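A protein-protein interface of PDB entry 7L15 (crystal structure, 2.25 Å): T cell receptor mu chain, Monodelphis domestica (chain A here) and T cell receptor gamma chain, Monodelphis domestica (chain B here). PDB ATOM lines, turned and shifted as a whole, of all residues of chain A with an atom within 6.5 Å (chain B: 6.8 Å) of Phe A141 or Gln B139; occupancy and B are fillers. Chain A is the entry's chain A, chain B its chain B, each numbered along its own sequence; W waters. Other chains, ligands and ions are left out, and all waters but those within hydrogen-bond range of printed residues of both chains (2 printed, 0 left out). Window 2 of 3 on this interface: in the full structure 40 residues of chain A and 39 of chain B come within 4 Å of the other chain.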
ATOM      1  N   SER A 139     -25.113   9.193  -7.261  1.00  0.00           N
ATOM      2  CA  SER A 139     -23.906   8.533  -7.736  1.00  0.00           C
ATOM      3  C   SER A 139     -24.148   7.029  -7.744  1.00  0.00           C
ATOM      4  O   SER A 139     -25.036   6.526  -7.051  1.00  0.00           O
ATOM      5  CB  SER A 139     -22.699   8.881  -6.858  1.00  0.00           C
ATOM      6  OG  SER A 139     -23.073   8.933  -5.492  1.00  0.00           O
ATOM      7  N   VAL A 140     -23.373   6.313  -8.563  1.00  0.00           N
ATOM      8  CA  VAL A 140     -23.626   4.901  -8.824  1.00  0.00           C
ATOM      9  C   VAL A 140     -22.331   4.115  -8.653  1.00  0.00           C
ATOM     10  O   VAL A 140     -21.312   4.445  -9.267  1.00  0.00           O
ATOM     11  CB  VAL A 140     -24.215   4.690 -10.232  1.00  0.00           C
ATOM     12  CG1 VAL A 140     -24.448   3.224 -10.502  1.00  0.00           C
ATOM     13  CG2 VAL A 140     -25.522   5.474 -10.371  1.00  0.00           C
ATOM     14  N   PHE A 141     -22.377   3.058  -7.843  1.00  0.00           N
ATOM     15  CA  PHE A 141     -21.208   2.235  -7.576  1.00  0.00           C
ATOM     16  C   PHE A 141     -21.564   0.776  -7.749  1.00  0.00           C
ATOM     17  O   PHE A 141     -22.598   0.329  -7.243  1.00  0.00           O
ATOM     18  CB  PHE A 141     -20.687   2.478  -6.161  1.00  0.00           C
ATOM     19  CG  PHE A 141     -20.500   3.925  -5.853  1.00  0.00           C
ATOM     20  CD1 PHE A 141     -19.341   4.586  -6.251  1.00  0.00           C
ATOM     21  CD2 PHE A 141     -21.482   4.637  -5.199  1.00  0.00           C
ATOM     22  CE1 PHE A 141     -19.175   5.954  -5.988  1.00  0.00           C
ATOM     23  CE2 PHE A 141     -21.315   6.001  -4.919  1.00  0.00           C
ATOM     24  CZ  PHE A 141     -20.156   6.655  -5.314  1.00  0.00           C
ATOM     25  N   LEU A 142     -20.699   0.033  -8.445  1.00  0.00           N
ATOM     26  CA  LEU A 142     -20.834  -1.413  -8.556  1.00  0.00           C
ATOM     27  C   LEU A 142     -20.007  -2.090  -7.474  1.00  0.00           C
ATOM     28  O   LEU A 142     -18.872  -1.687  -7.202  1.00  0.00           O
ATOM     29  CB  LEU A 142     -20.375  -1.903  -9.930  1.00  0.00           C
ATOM     30  CG  LEU A 142     -21.303  -1.744 -11.128  1.00  0.00           C
ATOM     31  CD1 LEU A 142     -20.532  -2.066 -12.402  1.00  0.00           C
ATOM     32  CD2 LEU A 142     -22.481  -2.681 -10.967  1.00  0.00           C
ATOM     33  N   VAL A 143     -20.583  -3.122  -6.854  1.00  0.00           N
ATOM     34  CA  VAL A 143     -19.878  -3.926  -5.868  1.00  0.00           C
ATOM     35  C   VAL A 143     -20.189  -5.383  -6.159  1.00  0.00           C
ATOM     36  O   VAL A 143     -21.304  -5.728  -6.562  1.00  0.00           O
ATOM     37  CB  VAL A 143     -20.275  -3.588  -4.412  1.00  0.00           C
ATOM     38  CG1 VAL A 143     -19.250  -4.194  -3.441  1.00  0.00           C
ATOM     39  CG2 VAL A 143     -20.421  -2.080  -4.216  1.00  0.00           C
ATOM     40  N   ALA A 150     -24.051  -6.073  -6.474  1.00  0.00           N
ATOM     41  CA  ALA A 150     -24.877  -5.029  -5.900  1.00  0.00           C
ATOM     42  C   ALA A 150     -24.569  -3.742  -6.636  1.00  0.00           C
ATOM     43  O   ALA A 150     -23.409  -3.427  -6.896  1.00  0.00           O
ATOM     44  CB  ALA A 150     -24.618  -4.847  -4.394  1.00  0.00           C
ATOM     45  N   CYS A 151     -25.606  -3.009  -6.986  1.00  0.00           N
ATOM     46  CA  CYS A 151     -25.453  -1.678  -7.536  1.00  0.00           C
ATOM     47  C   CYS A 151     -25.892  -0.691  -6.458  1.00  0.00           C
ATOM     48  O   CYS A 151     -27.052  -0.695  -6.052  1.00  0.00           O
ATOM     49  CB  CYS A 151     -26.268  -1.539  -8.825  1.00  0.00           C
ATOM     50  SG  CYS A 151     -26.196   0.076  -9.491  1.00  0.00           S
ATOM     51  N   LEU A 152     -24.962   0.127  -5.975  1.00  0.00           N
ATOM     52  CA  LEU A 152     -25.212   1.045  -4.871  1.00  0.00           C
ATOM     53  C   LEU A 152     -25.498   2.430  -5.433  1.00  0.00           C
ATOM     54  O   LEU A 152     -24.686   2.982  -6.181  1.00  0.00           O
ATOM     55  CB  LEU A 152     -24.010   1.082  -3.927  1.00  0.00           C
ATOM     56  CG  LEU A 152     -23.902   2.256  -2.964  1.00  0.00           C
ATOM     57  CD1 LEU A 152     -25.077   2.270  -2.041  1.00  0.00           C
ATOM     58  CD2 LEU A 152     -22.607   2.101  -2.152  1.00  0.00           C
ATOM     59  N   ILE A 153     -26.635   3.000  -5.051  1.00  0.00           N
ATOM     60  CA  ILE A 153     -27.133   4.248  -5.619  1.00  0.00           C
ATOM     61  C   ILE A 153     -27.363   5.222  -4.466  1.00  0.00           C
ATOM     62  O   ILE A 153     -28.294   5.031  -3.671  1.00  0.00           O
ATOM     63  CB  ILE A 153     -28.417   4.005  -6.417  1.00  0.00           C
ATOM     64  CG1 ILE A 153     -28.151   2.929  -7.467  1.00  0.00           C
ATOM     65  CG2 ILE A 153     -28.913   5.315  -7.064  1.00  0.00           C
ATOM     66  CD1 ILE A 153     -29.423   2.278  -7.989  1.00  0.00           C
ATOM     67  N   ARG A 154     -26.540   6.276  -4.371  1.00  0.00           N
ATOM     68  CA  ARG A 154     -26.464   7.072  -3.142  1.00  0.00           C
ATOM     69  C   ARG A 154     -26.948   8.501  -3.320  1.00  0.00           C
ATOM     70  O   ARG A 154     -26.475   9.230  -4.197  1.00  0.00           O
ATOM     71  CB  ARG A 154     -25.046   7.104  -2.582  1.00  0.00           C
ATOM     72  CG  ARG A 154     -24.586   5.759  -2.113  1.00  0.00           C
ATOM     73  CD  ARG A 154     -23.798   5.781  -0.814  1.00  0.00           C
ATOM     74  NE  ARG A 154     -23.846   7.047  -0.103  1.00  0.00           N
ATOM     75  CZ  ARG A 154     -22.776   7.676   0.370  1.00  0.00           C
ATOM     76  NH1 ARG A 154     -22.920   8.819   1.015  1.00  0.00           N
ATOM     77  NH2 ARG A 154     -21.562   7.149   0.222  1.00  0.00           N
ATOM     78  N   CYS A 203     -24.386  -1.092 -14.492  1.00  0.00           N
ATOM     79  CA  CYS A 203     -25.542  -0.612 -13.763  1.00  0.00           C
ATOM     80  C   CYS A 203     -25.926   0.745 -14.319  1.00  0.00           C
ATOM     81  O   CYS A 203     -25.089   1.647 -14.393  1.00  0.00           O
ATOM     82  CB  CYS A 203     -25.267  -0.505 -12.267  1.00  0.00           C
ATOM     83  SG  CYS A 203     -26.774  -0.068 -11.439  1.00  0.00           S
ATOM     84  N   MET A 214     -22.312   3.044 -13.955  1.00  0.00           N
ATOM     85  CA  MET A 214     -20.974   2.494 -13.785  1.00  0.00           C
ATOM     86  C   MET A 214     -20.922   1.129 -14.468  1.00  0.00           C
ATOM     87  O   MET A 214     -21.904   0.382 -14.454  1.00  0.00           O
ATOM     88  CB  MET A 214     -20.595   2.356 -12.297  1.00  0.00           C
ATOM     89  CG  MET A 214     -19.190   1.767 -12.070  1.00  0.00           C
ATOM     90  SD  MET A 214     -18.515   2.130 -10.423  1.00  0.00           S
ATOM     91  CE  MET A 214     -17.864   0.557  -9.892  1.00  0.00           C
ATOM     92  N   THR B 133     -16.278   0.148  -1.419  1.00  0.00           N
ATOM     93  CA  THR B 133     -15.361   0.203  -2.545  1.00  0.00           C
ATOM     94  C   THR B 133     -14.550   1.498  -2.518  1.00  0.00           C
ATOM     95  O   THR B 133     -15.006   2.535  -2.023  1.00  0.00           O
ATOM     96  CB  THR B 133     -16.098   0.112  -3.883  1.00  0.00           C
ATOM     97  OG1 THR B 133     -17.026   1.196  -3.981  1.00  0.00           O
ATOM     98  CG2 THR B 133     -16.849  -1.191  -3.999  1.00  0.00           C
ATOM     99  N   SER B 134     -13.339   1.419  -3.083  1.00  0.00           N
ATOM    100  CA  SER B 134     -12.445   2.571  -3.137  1.00  0.00           C
ATOM    101  C   SER B 134     -13.109   3.728  -3.862  1.00  0.00           C
ATOM    102  O   SER B 134     -13.070   4.876  -3.402  1.00  0.00           O
ATOM    103  CB  SER B 134     -11.136   2.193  -3.846  1.00  0.00           C
ATOM    104  OG  SER B 134     -10.474   1.123  -3.191  1.00  0.00           O
ATOM    105  N   GLU B 135     -13.738   3.432  -5.001  1.00  0.00           N
ATOM    106  CA  GLU B 135     -14.414   4.471  -5.766  1.00  0.00           C
ATOM    107  C   GLU B 135     -15.465   5.200  -4.927  1.00  0.00           C
ATOM    108  O   GLU B 135     -15.576   6.433  -4.991  1.00  0.00           O
ATOM    109  CB  GLU B 135     -15.041   3.861  -7.021  1.00  0.00           C
ATOM    110  CG  GLU B 135     -15.320   4.880  -8.105  1.00  0.00           C
ATOM    111  CD  GLU B 135     -14.079   5.685  -8.479  1.00  0.00           C
ATOM    112  OE1 GLU B 135     -12.979   5.101  -8.538  1.00  0.00           O
ATOM    113  OE2 GLU B 135     -14.206   6.909  -8.711  1.00  0.00           O
ATOM    114  N   GLU B 136     -16.241   4.459  -4.124  1.00  0.00           N
ATOM    115  CA  GLU B 136     -17.215   5.113  -3.260  1.00  0.00           C
ATOM    116  C   GLU B 136     -16.517   6.052  -2.279  1.00  0.00           C
ATOM    117  O   GLU B 136     -16.941   7.197  -2.083  1.00  0.00           O
ATOM    118  CB  GLU B 136     -18.077   4.087  -2.500  1.00  0.00           C
ATOM    119  CG  GLU B 136     -19.152   4.811  -1.665  1.00  0.00           C
ATOM    120  CD  GLU B 136     -19.928   3.939  -0.681  1.00  0.00           C
ATOM    121  OE1 GLU B 136     -19.585   2.758  -0.522  1.00  0.00           O
ATOM    122  OE2 GLU B 136     -20.893   4.455  -0.060  1.00  0.00           O
ATOM    123  N   ILE B 137     -15.443   5.578  -1.645  1.00  0.00           N
ATOM    124  CA  ILE B 137     -14.723   6.417  -0.688  1.00  0.00           C
ATOM    125  C   ILE B 137     -14.122   7.625  -1.388  1.00  0.00           C
ATOM    126  O   ILE B 137     -14.127   8.738  -0.854  1.00  0.00           O
ATOM    127  CB  ILE B 137     -13.637   5.599   0.031  1.00  0.00           C
ATOM    128  CG1 ILE B 137     -14.281   4.544   0.931  1.00  0.00           C
ATOM    129  CG2 ILE B 137     -12.776   6.508   0.838  1.00  0.00           C
ATOM    130  CD1 ILE B 137     -13.518   3.236   0.934  1.00  0.00           C
ATOM    131  N   LYS B 138     -13.589   7.422  -2.590  1.00  0.00           N
ATOM    132  CA  LYS B 138     -13.020   8.530  -3.349  1.00  0.00           C
ATOM    133  C   LYS B 138     -14.079   9.570  -3.694  1.00  0.00           C
ATOM    134  O   LYS B 138     -13.831  10.774  -3.584  1.00  0.00           O
ATOM    135  CB  LYS B 138     -12.357   7.997  -4.618  1.00  0.00           C
ATOM    136  CG  LYS B 138     -11.699   9.060  -5.478  1.00  0.00           C
ATOM    137  CD  LYS B 138     -11.991   8.810  -6.962  1.00  0.00           C
ATOM    138  CE  LYS B 138     -10.779   9.086  -7.836  1.00  0.00           C
ATOM    139  NZ  LYS B 138     -10.256  10.472  -7.667  1.00  0.00           N
ATOM    140  N   GLN B 139     -15.275   9.132  -4.096  1.00  0.00           N
ATOM    141  CA  GLN B 139     -16.270  10.105  -4.535  1.00  0.00           C
ATOM    142  C   GLN B 139     -17.086  10.688  -3.383  1.00  0.00           C
ATOM    143  O   GLN B 139     -17.579  11.810  -3.500  1.00  0.00           O
ATOM    144  CB  GLN B 139     -17.218   9.482  -5.559  1.00  0.00           C
ATOM    145  CG  GLN B 139     -16.606   9.085  -6.896  1.00  0.00           C
ATOM    146  CD  GLN B 139     -17.662   8.535  -7.880  1.00  0.00           C
ATOM    147  OE1 GLN B 139     -17.435   7.529  -8.555  1.00  0.00           O
ATOM    148  NE2 GLN B 139     -18.815   9.199  -7.954  1.00  0.00           N
ATOM    149  N   LYS B 140     -17.271   9.963  -2.279  1.00  0.00           N
ATOM    150  CA  LYS B 140     -18.198  10.424  -1.258  1.00  0.00           C
ATOM    151  C   LYS B 140     -17.598  10.546   0.127  1.00  0.00           C
ATOM    152  O   LYS B 140     -18.337  10.872   1.059  1.00  0.00           O
ATOM    153  CB  LYS B 140     -19.421   9.496  -1.157  1.00  0.00           C
ATOM    154  CG  LYS B 140     -20.133   9.204  -2.483  1.00  0.00           C
ATOM    155  CD  LYS B 140     -20.944  10.393  -2.997  1.00  0.00           C
ATOM    156  CE  LYS B 140     -22.250  10.576  -2.233  1.00  0.00           C
ATOM    157  NZ  LYS B 140     -23.279  11.118  -3.163  1.00  0.00           N
ATOM    158  N   GLN B 141     -16.305  10.272   0.307  1.00  0.00           N
ATOM    159  CA  GLN B 141     -15.695  10.352   1.635  1.00  0.00           C
ATOM    160  C   GLN B 141     -16.466   9.528   2.648  1.00  0.00           C
ATOM    161  O   GLN B 141     -16.547   9.890   3.817  1.00  0.00           O
ATOM    162  CB  GLN B 141     -15.603  11.786   2.133  1.00  0.00           C
ATOM    163  CG  GLN B 141     -14.491  12.579   1.546  1.00  0.00           C
ATOM    164  CD  GLN B 141     -14.288  13.868   2.293  1.00  0.00           C
ATOM    165  OE1 GLN B 141     -13.299  14.035   2.984  1.00  0.00           O
ATOM    166  NE2 GLN B 141     -15.242  14.782   2.173  1.00  0.00           N
ATOM    167  N   SER B 142     -17.075   8.444   2.195  1.00  0.00           N
ATOM    168  CA  SER B 142     -17.842   7.576   3.073  1.00  0.00           C
ATOM    169  C   SER B 142     -17.971   6.225   2.385  1.00  0.00           C
ATOM    170  O   SER B 142     -17.729   6.097   1.182  1.00  0.00           O
ATOM    171  CB  SER B 142     -19.213   8.183   3.406  1.00  0.00           C
ATOM    172  OG  SER B 142     -19.902   8.631   2.250  1.00  0.00           O
ATOM    173  N   THR B 144     -20.101   2.252   2.233  1.00  0.00           N
ATOM    174  CA  THR B 144     -21.349   1.546   2.498  1.00  0.00           C
ATOM    175  C   THR B 144     -21.091   0.046   2.618  1.00  0.00           C
ATOM    176  O   THR B 144     -20.567  -0.581   1.691  1.00  0.00           O
ATOM    177  CB  THR B 144     -22.380   1.820   1.403  1.00  0.00           C
ATOM    178  OG1 THR B 144     -22.577   3.235   1.279  1.00  0.00           O
ATOM    179  CG2 THR B 144     -23.716   1.164   1.746  1.00  0.00           C
HETATM  180  O   HOH W   1     -21.244   7.952 -10.016  1.00  0.00           O
HETATM  181  O   HOH W   2     -22.181  12.137  -5.928  1.00  0.00           O
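Water W1 bridges the backbone NH (N) of Val A140 (3.1 Å) and the side-chain amide nitrogen (NE2) of Gln B139 (3.4 Å). Water W2 bridges the side-chain amino group (NZ) of Lys B140 (3.1 Å) and the side-chain hydroxyl (OG) of Ser A139 (3.4 Å).
The side-chain sulfur of Met A214 sits close to the backbone NH of Leu A142 (3.6 Å). The backbone carbonyl oxygen of Val A143 sits at hydrogen-bond distance from the backbone NH of Ala A150. The backbone NH of Glu B136 lies within hydrogen-bond range of the side-chain hydroxyl of Thr B133, at 3.4 Å. OE2 of Glu B135 sits close to OE1 of Gln B139, at 3.3 Å. The side-chain hydroxyl of Thr B144 is in hydrogen-bond range of the side-chain carboxylate of Glu B136. The side-chain sulfur of Cys A203 is disulfide-bonded to the side-chain sulfur of Cys A151, at 2.0 Å.
Among the printed residues, merely in contact across the chains: Phe A141 with Glu B136 (3.5 Å), Arg A154 with Lys B140 (3.5 Å), Phe A141 with Gln B139 (3.5 Å), Leu A152 with Glu B136 (3.5 Å), Arg A154 with Thr B144 (3.5 Å), Leu A152 with Thr B144 (3.6 Å), Val A143 with Thr B133 (3.7 Å), Phe A141 with Glu B135 (3.8 Å), Phe A141 with Lys B140 (3.8 Å) and Leu A142 with Thr B133 (3.8 Å).
Printed residues of chain A that touch a printed residue of chain B: Ser A139, Phe A141, Leu A142, Val A143, Leu A152 and Arg A154. Printed residues of chain B that touch a printed residue of chain A: Thr B133, Glu B135, Glu B136, Gln B139, Lys B140, Ser B142 and Thr B144. Among the printed residues, 13 pairs touch across the chains.
Printed residues of chain B within 4 Å of Ser A139: Lys B140. Val A140 touches none of the printed residues of chain B. Phe A141 touches just these residues of chain B: Glu B135 (3.8 Å), Glu B136 (3.5 Å), Gln B139 (3.5 Å) and Lys B140 (3.8 Å). Ala A150 touches none of the printed residues of chain B. Of the printed residues of chain B, Arg A154 touches Glu B136, Lys B140, Ser B142 and Thr B144. Printed residues of chain A within 4 Å of Thr B133: Leu A142 and Val A143. Gln B139 touches just one residue of chain A: Phe A141. Printed residues of chain A within 4 Å of Lys B140: Ser A139, Phe A141 and Arg A154. The nearest residue of chain B that does not touch Phe A141 is Thr B133 (4.4 Å). The nearest residue of chain A that does not touch Gln B139 is Ser A139 (4.05 Å).
The side-chain hydroxyl of Ser A139 sits at hydrogen-bond distance from the side-chain amino group of Lys B140 (3.2 Å). OE2 of Glu B136 is in salt-bridge range of NH2 of Arg A154. NH2 of Arg A154 sits at hydrogen-bond distance from OG of Ser B142 (3.0 Å).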
